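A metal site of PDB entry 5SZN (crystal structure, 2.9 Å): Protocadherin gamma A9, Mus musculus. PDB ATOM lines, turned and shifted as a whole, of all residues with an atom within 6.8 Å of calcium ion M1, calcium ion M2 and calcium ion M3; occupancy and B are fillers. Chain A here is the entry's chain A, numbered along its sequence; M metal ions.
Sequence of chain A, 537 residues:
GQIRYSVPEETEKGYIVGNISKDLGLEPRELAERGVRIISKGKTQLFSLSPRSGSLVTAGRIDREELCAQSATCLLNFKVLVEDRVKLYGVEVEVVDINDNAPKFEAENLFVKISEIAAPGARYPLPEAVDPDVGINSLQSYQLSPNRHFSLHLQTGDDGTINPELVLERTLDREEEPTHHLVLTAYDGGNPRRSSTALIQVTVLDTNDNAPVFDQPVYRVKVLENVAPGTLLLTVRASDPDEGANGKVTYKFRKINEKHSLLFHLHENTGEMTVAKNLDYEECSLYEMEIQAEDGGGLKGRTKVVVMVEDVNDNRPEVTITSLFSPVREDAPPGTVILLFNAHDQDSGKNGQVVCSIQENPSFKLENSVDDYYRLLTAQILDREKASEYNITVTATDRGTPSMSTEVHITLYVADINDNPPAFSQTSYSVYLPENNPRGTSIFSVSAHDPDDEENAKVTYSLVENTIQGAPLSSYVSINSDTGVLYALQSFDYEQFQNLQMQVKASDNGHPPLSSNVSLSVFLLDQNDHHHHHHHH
Of the 26 residues printed, 7 come within 4 Å of calcium ion M2. Along chain A the residues within 4 Å of calcium ion M2 span positions 225 to 347. The nearest printed residue that does not touch calcium ion M2 is Asn 313 (4.9 Å).
OD1 of Asp 314 lies close to ND2 of Asn 315 (2.8 Å). The side-chain carboxylate (OE1) of Glu 225 sits close to the backbone NH (N) of Tyr 281 (2.8 Å). SD of Met 404 sits close to N of Asn 315 (3.8 Å). O of Glu 310 sits at hydrogen-bond distance from N of Glu 225 (3.4 Å). N of Met 404 is in hydrogen-bond range of OD1 of Asp 398, 2.7 Å away. OD2 of Asp 311 is in hydrogen-bond range of N of Ser 348 (3.4 Å). The side-chain amide oxygen (OD1) of Asn 315 sits close to the side-chain amide oxygen (OE1) of Gln 346 (2.8 Å). OD2 of Asp 311 is in hydrogen-bond range of ND2 of Asn 351 (3.4 Å).
Within 4 Å of calcium ion M1: Asn 313, Asn 315, Asp 345, Asp 347, Asn 351 and Asp 398. The nearest printed residue that does not touch calcium ion M1 is Arg 316 (4.7 Å).
Calcium ion M2 is bound by the side-chain carboxylate of Glu 225, the side-chain carboxylate of Asp 314, the side-chain carboxylate of Glu 282, the side-chain carboxylate of Asp 347, the backbone carbonyl oxygen of Val 312 and the side-chain carboxylate of Asp 311. Slightly farther from calcium ion M2 lies the side-chain amide nitrogen (ND2) of Asn 315 (3.1 Å).
Five residues have an atom within 4 Å of calcium ion M3: Glu 225, Asp 280, Glu 282, Asp 314 and Asn 315. The nearest printed residue that does not touch calcium ion M3 is Tyr 281 (4.7 Å).
Calcium ion M3 is bound by OD1 of Asp 280 (2.4 Å), OD2 of Asp 314 (2.4 Å) and OE1 of Glu 225 (2.7 Å). Slightly farther from calcium ion M3 lies OD1 of Asp 314 (2.9 Å). Slightly farther from calcium ion M3 lies the side-chain carboxylate (OE1) of Glu 282 (3.0 Å).
Calcium ion M1 is bound by the side-chain carboxylate (OD2) of Asp 347 (2.3 Å), the side-chain carboxylate (OD2) of Asp 345 (2.4 Å), the backbone carbonyl oxygen (O) of Asn 351 (2.6 Å), the side-chain amide oxygen (OD1) of Asn 313 (2.7 Å) and the backbone carbonyl oxygen (O) of Asn 315 (2.8 Å). Calcium ion M1 has five donor atoms within binding distance. Slightly farther from calcium ion M1 lies OD1 of Asp 345 (2.9 Å). Slightly farther from calcium ion M1 lies OD2 of Asp 398 (3.0 Å).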
ATOM      1  N   GLU A 225      24.598 -15.268 -21.935  1.00  0.00           N
ATOM      2  CA  GLU A 225      23.612 -15.455 -20.884  1.00  0.00           C
ATOM      3  C   GLU A 225      22.222 -15.760 -21.434  1.00  0.00           C
ATOM      4  O   GLU A 225      21.417 -16.406 -20.750  1.00  0.00           O
ATOM      5  CB  GLU A 225      23.554 -14.209 -19.983  1.00  0.00           C
ATOM      6  CG  GLU A 225      23.361 -12.896 -20.728  1.00  0.00           C
ATOM      7  CD  GLU A 225      23.250 -11.707 -19.798  1.00  0.00           C
ATOM      8  OE1 GLU A 225      22.912 -11.904 -18.617  1.00  0.00           O
ATOM      9  OE2 GLU A 225      23.512 -10.567 -20.250  1.00  0.00           O
ATOM     10  N   ASN A 226      21.927 -15.330 -22.662  1.00  0.00           N
ATOM     11  CA  ASN A 226      20.630 -15.558 -23.271  1.00  0.00           C
ATOM     12  C   ASN A 226      20.476 -16.997 -23.732  1.00  0.00           C
ATOM     13  O   ASN A 226      19.631 -17.306 -24.585  1.00  0.00           O
ATOM     14  CB  ASN A 226      20.428 -14.602 -24.443  1.00  0.00           C
ATOM     15  CG  ASN A 226      21.574 -14.663 -25.447  1.00  0.00           C
ATOM     16  OD1 ASN A 226      22.353 -15.611 -25.458  1.00  0.00           O
ATOM     17  ND2 ASN A 226      21.655 -13.651 -26.297  1.00  0.00           N
ATOM     18  N   LEU A 279      20.344 -18.619 -17.641  1.00  0.00           N
ATOM     19  CA  LEU A 279      21.486 -18.033 -16.956  1.00  0.00           C
ATOM     20  C   LEU A 279      21.398 -16.507 -16.977  1.00  0.00           C
ATOM     21  O   LEU A 279      20.609 -15.909 -17.701  1.00  0.00           O
ATOM     22  CB  LEU A 279      22.797 -18.500 -17.579  1.00  0.00           C
ATOM     23  CG  LEU A 279      23.103 -19.990 -17.452  1.00  0.00           C
ATOM     24  CD1 LEU A 279      24.442 -20.328 -18.085  1.00  0.00           C
ATOM     25  CD2 LEU A 279      23.077 -20.417 -15.983  1.00  0.00           C
ATOM     26  N   ASP A 280      22.251 -15.891 -16.163  1.00  0.00           N
ATOM     27  CA  ASP A 280      22.266 -14.429 -16.036  1.00  0.00           C
ATOM     28  C   ASP A 280      23.679 -13.984 -15.694  1.00  0.00           C
ATOM     29  O   ASP A 280      24.222 -14.364 -14.655  1.00  0.00           O
ATOM     30  CB  ASP A 280      21.288 -13.975 -14.958  1.00  0.00           C
ATOM     31  CG  ASP A 280      20.963 -12.500 -15.060  1.00  0.00           C
ATOM     32  OD1 ASP A 280      20.927 -11.974 -16.186  1.00  0.00           O
ATOM     33  OD2 ASP A 280      20.738 -11.871 -14.004  1.00  0.00           O
ATOM     34  N   TYR A 281      24.274 -13.171 -16.581  1.00  0.00           N
ATOM     35  CA  TYR A 281      25.628 -12.678 -16.351  1.00  0.00           C
ATOM     36  C   TYR A 281      25.725 -11.866 -15.071  1.00  0.00           C
ATOM     37  O   TYR A 281      26.772 -11.882 -14.410  1.00  0.00           O
ATOM     38  CB  TYR A 281      26.080 -11.841 -17.550  1.00  0.00           C
ATOM     39  CG  TYR A 281      27.501 -11.302 -17.450  1.00  0.00           C
ATOM     40  CD1 TYR A 281      28.573 -12.042 -17.935  1.00  0.00           C
ATOM     41  CD2 TYR A 281      27.758 -10.063 -16.896  1.00  0.00           C
ATOM     42  CE1 TYR A 281      29.869 -11.564 -17.848  1.00  0.00           C
ATOM     43  CE2 TYR A 281      29.045  -9.571 -16.814  1.00  0.00           C
ATOM     44  CZ  TYR A 281      30.092 -10.324 -17.293  1.00  0.00           C
ATOM     45  OH  TYR A 281      31.379  -9.843 -17.203  1.00  0.00           O
ATOM     46  N   GLU A 282      24.664 -11.166 -14.702  1.00  0.00           N
ATOM     47  CA  GLU A 282      24.705 -10.318 -13.514  1.00  0.00           C
ATOM     48  C   GLU A 282      24.594 -11.130 -12.230  1.00  0.00           C
ATOM     49  O   GLU A 282      25.126 -10.721 -11.197  1.00  0.00           O
ATOM     50  CB  GLU A 282      23.587  -9.270 -13.570  1.00  0.00           C
ATOM     51  CG  GLU A 282      23.749  -8.251 -14.689  1.00  0.00           C
ATOM     52  CD  GLU A 282      23.384  -8.797 -16.053  1.00  0.00           C
ATOM     53  OE1 GLU A 282      22.703  -9.839 -16.121  1.00  0.00           O
ATOM     54  OE2 GLU A 282      23.777  -8.182 -17.067  1.00  0.00           O
ATOM     55  N   GLU A 310      29.049 -14.642 -20.710  1.00  0.00           N
ATOM     56  CA  GLU A 310      29.380 -13.303 -21.151  1.00  0.00           C
ATOM     57  C   GLU A 310      28.106 -12.464 -21.233  1.00  0.00           C
ATOM     58  O   GLU A 310      27.013 -12.995 -21.448  1.00  0.00           O
ATOM     59  CB  GLU A 310      30.104 -13.306 -22.499  1.00  0.00           C
ATOM     60  CG  GLU A 310      31.438 -14.036 -22.472  1.00  0.00           C
ATOM     61  CD  GLU A 310      32.465 -13.347 -21.584  1.00  0.00           C
ATOM     62  OE1 GLU A 310      32.940 -12.264 -21.954  1.00  0.00           O
ATOM     63  OE2 GLU A 310      32.784 -13.905 -20.512  1.00  0.00           O
ATOM     64  N   ASP A 311      28.260 -11.159 -21.071  1.00  0.00           N
ATOM     65  CA  ASP A 311      27.115 -10.269 -20.942  1.00  0.00           C
ATOM     66  C   ASP A 311      26.412 -10.073 -22.278  1.00  0.00           C
ATOM     67  O   ASP A 311      27.023 -10.156 -23.349  1.00  0.00           O
ATOM     68  CB  ASP A 311      27.560  -8.926 -20.367  1.00  0.00           C
ATOM     69  CG  ASP A 311      26.408  -7.951 -20.211  1.00  0.00           C
ATOM     70  OD1 ASP A 311      25.527  -8.197 -19.363  1.00  0.00           O
ATOM     71  OD2 ASP A 311      26.391  -6.932 -20.943  1.00  0.00           O
ATOM     72  N   VAL A 312      25.104  -9.812 -22.210  1.00  0.00           N
ATOM     73  CA  VAL A 312      24.283  -9.552 -23.381  1.00  0.00           C
ATOM     74  C   VAL A 312      23.382  -8.364 -23.070  1.00  0.00           C
ATOM     75  O   VAL A 312      22.909  -8.204 -21.936  1.00  0.00           O
ATOM     76  CB  VAL A 312      23.444 -10.787 -23.792  1.00  0.00           C
ATOM     77  CG1 VAL A 312      22.513 -10.467 -24.950  1.00  0.00           C
ATOM     78  CG2 VAL A 312      24.358 -11.933 -24.164  1.00  0.00           C
ATOM     79  N   ASN A 313      23.157  -7.503 -24.069  1.00  0.00           N
ATOM     80  CA  ASN A 313      22.257  -6.372 -23.916  1.00  0.00           C
ATOM     81  C   ASN A 313      20.804  -6.817 -23.767  1.00  0.00           C
ATOM     82  O   ASN A 313      20.074  -6.863 -24.752  1.00  0.00           O
ATOM     83  CB  ASN A 313      22.396  -5.416 -25.101  1.00  0.00           C
ATOM     84  CG  ASN A 313      21.716  -4.079 -24.868  1.00  0.00           C
ATOM     85  OD1 ASN A 313      21.464  -3.699 -23.727  1.00  0.00           O
ATOM     86  ND2 ASN A 313      21.427  -3.361 -25.944  1.00  0.00           N
ATOM     87  N   ASP A 314      20.390  -7.160 -22.542  1.00  0.00           N
ATOM     88  CA  ASP A 314      19.017  -7.535 -22.237  1.00  0.00           C
ATOM     89  C   ASP A 314      18.451  -6.707 -21.103  1.00  0.00           C
ATOM     90  O   ASP A 314      17.561  -7.156 -20.370  1.00  0.00           O
ATOM     91  CB  ASP A 314      18.911  -9.030 -21.925  1.00  0.00           C
ATOM     92  CG  ASP A 314      19.633  -9.410 -20.646  1.00  0.00           C
ATOM     93  OD1 ASP A 314      20.648  -8.762 -20.324  1.00  0.00           O
ATOM     94  OD2 ASP A 314      19.196 -10.364 -19.960  1.00  0.00           O
ATOM     95  N   ASN A 315      18.974  -5.500 -20.915  1.00  0.00           N
ATOM     96  CA  ASN A 315      18.525  -4.591 -19.869  1.00  0.00           C
ATOM     97  C   ASN A 315      18.456  -3.182 -20.426  1.00  0.00           C
ATOM     98  O   ASN A 315      19.191  -2.819 -21.346  1.00  0.00           O
ATOM     99  CB  ASN A 315      19.455  -4.637 -18.655  1.00  0.00           C
ATOM    100  CG  ASN A 315      19.421  -5.966 -17.936  1.00  0.00           C
ATOM    101  OD1 ASN A 315      18.599  -6.181 -17.048  1.00  0.00           O
ATOM    102  ND2 ASN A 315      20.302  -6.877 -18.334  1.00  0.00           N
ATOM    103  N   ARG A 316      17.537  -2.363 -19.839  1.00  0.00           N
ATOM    104  CA  ARG A 316      17.266  -0.987 -20.219  1.00  0.00           C
ATOM    105  C   ARG A 316      17.919  -0.014 -19.239  1.00  0.00           C
ATOM    106  O   ARG A 316      18.099  -0.327 -18.062  1.00  0.00           O
ATOM    107  CB  ARG A 316      15.762  -0.727 -20.258  1.00  0.00           C
ATOM    108  CG  ARG A 316      15.103  -1.099 -21.573  1.00  0.00           C
ATOM    109  CD  ARG A 316      13.643  -0.676 -21.578  1.00  0.00           C
ATOM    110  NE  ARG A 316      13.054  -0.785 -22.906  1.00  0.00           N
ATOM    111  CZ  ARG A 316      12.518  -1.899 -23.393  1.00  0.00           C
ATOM    112  NH1 ARG A 316      12.505  -3.002 -22.665  1.00  0.00           N
ATOM    113  NH2 ARG A 316      12.002  -1.901 -24.620  1.00  0.00           N
ATOM    114  N   PRO A 317      18.287   1.176 -19.717  1.00  0.00           N
ATOM    115  CA  PRO A 317      18.862   2.181 -18.824  1.00  0.00           C
ATOM    116  C   PRO A 317      17.848   2.629 -17.778  1.00  0.00           C
ATOM    117  O   PRO A 317      16.640   2.626 -18.018  1.00  0.00           O
ATOM    118  CB  PRO A 317      19.246   3.325 -19.760  1.00  0.00           C
ATOM    119  CG  PRO A 317      19.346   2.692 -21.117  1.00  0.00           C
ATOM    120  CD  PRO A 317      18.317   1.608 -21.122  1.00  0.00           C
ATOM    121  N   ASP A 345      23.024   1.831 -16.230  1.00  0.00           N
ATOM    122  CA  ASP A 345      22.627   0.593 -16.888  1.00  0.00           C
ATOM    123  C   ASP A 345      23.168  -0.600 -16.097  1.00  0.00           C
ATOM    124  O   ASP A 345      24.249  -0.529 -15.508  1.00  0.00           O
ATOM    125  CB  ASP A 345      23.129   0.535 -18.334  1.00  0.00           C
ATOM    126  CG  ASP A 345      22.409  -0.508 -19.165  1.00  0.00           C
ATOM    127  OD1 ASP A 345      22.106  -1.606 -18.651  1.00  0.00           O
ATOM    128  OD2 ASP A 345      22.142  -0.227 -20.362  1.00  0.00           O
ATOM    129  N   GLN A 346      22.390  -1.687 -16.088  1.00  0.00           N
ATOM    130  CA  GLN A 346      22.824  -2.891 -15.392  1.00  0.00           C
ATOM    131  C   GLN A 346      23.873  -3.660 -16.183  1.00  0.00           C
ATOM    132  O   GLN A 346      24.707  -4.341 -15.594  1.00  0.00           O
ATOM    133  CB  GLN A 346      21.621  -3.800 -15.122  1.00  0.00           C
ATOM    134  CG  GLN A 346      20.488  -3.117 -14.361  1.00  0.00           C
ATOM    135  CD  GLN A 346      19.308  -4.043 -14.134  1.00  0.00           C
ATOM    136  OE1 GLN A 346      19.355  -5.228 -14.490  1.00  0.00           O
ATOM    137  NE2 GLN A 346      18.251  -3.515 -13.539  1.00  0.00           N
ATOM    138  N   ASP A 347      23.852  -3.543 -17.507  1.00  0.00           N
ATOM    139  CA  ASP A 347      24.796  -4.263 -18.351  1.00  0.00           C
ATOM    140  C   ASP A 347      26.201  -3.688 -18.209  1.00  0.00           C
ATOM    141  O   ASP A 347      26.419  -2.651 -17.579  1.00  0.00           O
ATOM    142  CB  ASP A 347      24.345  -4.223 -19.805  1.00  0.00           C
ATOM    143  CG  ASP A 347      23.035  -4.953 -20.035  1.00  0.00           C
ATOM    144  OD1 ASP A 347      22.807  -5.989 -19.376  1.00  0.00           O
ATOM    145  OD2 ASP A 347      22.233  -4.493 -20.882  1.00  0.00           O
ATOM    146  N   SER A 348      27.156  -4.371 -18.817  1.00  0.00           N
ATOM    147  CA  SER A 348      28.564  -3.983 -18.770  1.00  0.00           C
ATOM    148  C   SER A 348      29.047  -3.634 -20.175  1.00  0.00           C
ATOM    149  O   SER A 348      28.423  -3.981 -21.179  1.00  0.00           O
ATOM    150  CB  SER A 348      29.419  -5.105 -18.185  1.00  0.00           C
ATOM    151  OG  SER A 348      28.921  -5.537 -16.926  1.00  0.00           O
ATOM    152  N   LYS A 350      30.018  -1.855 -23.651  1.00  0.00           N
ATOM    153  CA  LYS A 350      29.231  -1.046 -24.585  1.00  0.00           C
ATOM    154  C   LYS A 350      27.738  -1.196 -24.353  1.00  0.00           C
ATOM    155  O   LYS A 350      26.970  -0.324 -24.784  1.00  0.00           O
ATOM    156  CB  LYS A 350      29.582  -1.433 -26.024  1.00  0.00           C
ATOM    157  N   ASN A 351      27.301  -2.274 -23.708  1.00  0.00           N
ATOM    158  CA  ASN A 351      25.905  -2.413 -23.316  1.00  0.00           C
ATOM    159  C   ASN A 351      25.558  -1.636 -22.058  1.00  0.00           C
ATOM    160  O   ASN A 351      24.372  -1.505 -21.731  1.00  0.00           O
ATOM    161  CB  ASN A 351      25.569  -3.896 -23.119  1.00  0.00           C
ATOM    162  CG  ASN A 351      25.836  -4.742 -24.352  1.00  0.00           C
ATOM    163  OD1 ASN A 351      25.553  -4.321 -25.478  1.00  0.00           O
ATOM    164  ND2 ASN A 351      26.380  -5.938 -24.147  1.00  0.00           N
ATOM    165  N   GLY A 352      26.556  -1.119 -21.337  1.00  0.00           N
ATOM    166  CA  GLY A 352      26.326  -0.391 -20.115  1.00  0.00           C
ATOM    167  C   GLY A 352      26.496   1.105 -20.256  1.00  0.00           C
ATOM    168  O   GLY A 352      26.036   1.879 -19.419  1.00  0.00           O
ATOM    169  N   GLN A 353      27.176   1.538 -21.328  1.00  0.00           N
ATOM    170  CA  GLN A 353      27.323   2.963 -21.590  1.00  0.00           C
ATOM    171  C   GLN A 353      25.986   3.555 -22.011  1.00  0.00           C
ATOM    172  O   GLN A 353      25.230   2.957 -22.790  1.00  0.00           O
ATOM    173  CB  GLN A 353      28.371   3.205 -22.673  1.00  0.00           C
ATOM    174  CG  GLN A 353      29.770   2.762 -22.279  1.00  0.00           C
ATOM    175  CD  GLN A 353      30.783   3.049 -23.375  1.00  0.00           C
ATOM    176  OE1 GLN A 353      30.493   3.719 -24.353  1.00  0.00           O
ATOM    177  NE2 GLN A 353      31.988   2.515 -23.211  1.00  0.00           N
ATOM    178  N   ASP A 398      21.167   3.175 -24.736  1.00  0.00           N
ATOM    179  CA  ASP A 398      22.473   2.581 -24.486  1.00  0.00           C
ATOM    180  C   ASP A 398      23.257   2.470 -25.786  1.00  0.00           C
ATOM    181  O   ASP A 398      22.709   2.569 -26.890  1.00  0.00           O
ATOM    182  CB  ASP A 398      22.351   1.221 -23.796  1.00  0.00           C
ATOM    183  CG  ASP A 398      21.523   0.214 -24.587  1.00  0.00           C
ATOM    184  OD1 ASP A 398      21.282   0.413 -25.795  1.00  0.00           O
ATOM    185  OD2 ASP A 398      21.111  -0.808 -23.983  1.00  0.00           O
ATOM    186  N   ARG A 399      24.564   2.253 -25.655  1.00  0.00           N
ATOM    187  CA  ARG A 399      25.466   2.210 -26.791  1.00  0.00           C
ATOM    188  C   ARG A 399      25.683   0.794 -27.324  1.00  0.00           C
ATOM    189  O   ARG A 399      26.512   0.605 -28.227  1.00  0.00           O
ATOM    190  CB  ARG A 399      26.809   2.847 -26.417  1.00  0.00           C
ATOM    191  CG  ARG A 399      27.491   3.580 -27.568  1.00  0.00           C
ATOM    192  CD  ARG A 399      28.859   4.101 -27.146  1.00  0.00           C
ATOM    193  NE  ARG A 399      28.777   5.126 -26.114  1.00  0.00           N
ATOM    194  CZ  ARG A 399      28.746   6.432 -26.360  1.00  0.00           C
ATOM    195  NH1 ARG A 399      28.771   6.879 -27.612  1.00  0.00           N
ATOM    196  NH2 ARG A 399      28.678   7.295 -25.358  1.00  0.00           N
ATOM    197  N   GLY A 400      24.958  -0.199 -26.807  1.00  0.00           N
ATOM    198  CA  GLY A 400      25.114  -1.567 -27.249  1.00  0.00           C
ATOM    199  C   GLY A 400      24.319  -1.883 -28.502  1.00  0.00           C
ATOM    200  O   GLY A 400      23.682  -1.016 -29.113  1.00  0.00           O
ATOM    201  N   MET A 404      18.847  -0.341 -26.625  1.00  0.00           N
ATOM    202  CA  MET A 404      17.641  -0.239 -25.818  1.00  0.00           C
ATOM    203  C   MET A 404      17.562   1.147 -25.216  1.00  0.00           C
ATOM    204  O   MET A 404      18.503   1.602 -24.562  1.00  0.00           O
ATOM    205  CB  MET A 404      17.620  -1.295 -24.707  1.00  0.00           C
ATOM    206  CG  MET A 404      17.481  -2.727 -25.193  1.00  0.00           C
ATOM    207  SD  MET A 404      17.218  -3.872 -23.817  1.00  0.00           S
ATOM    208  CE  MET A 404      16.993  -5.412 -24.708  1.00  0.00           C
HETATM  209 CA    CA M   1      21.910  -2.316 -21.477  1.00  0.00          CA
HETATM  210 CA    CA M   2      22.807  -8.538 -19.258  1.00  0.00          CA
HETATM  211 CA    CA M   3      20.597 -10.618 -18.080  1.00  0.00          CA
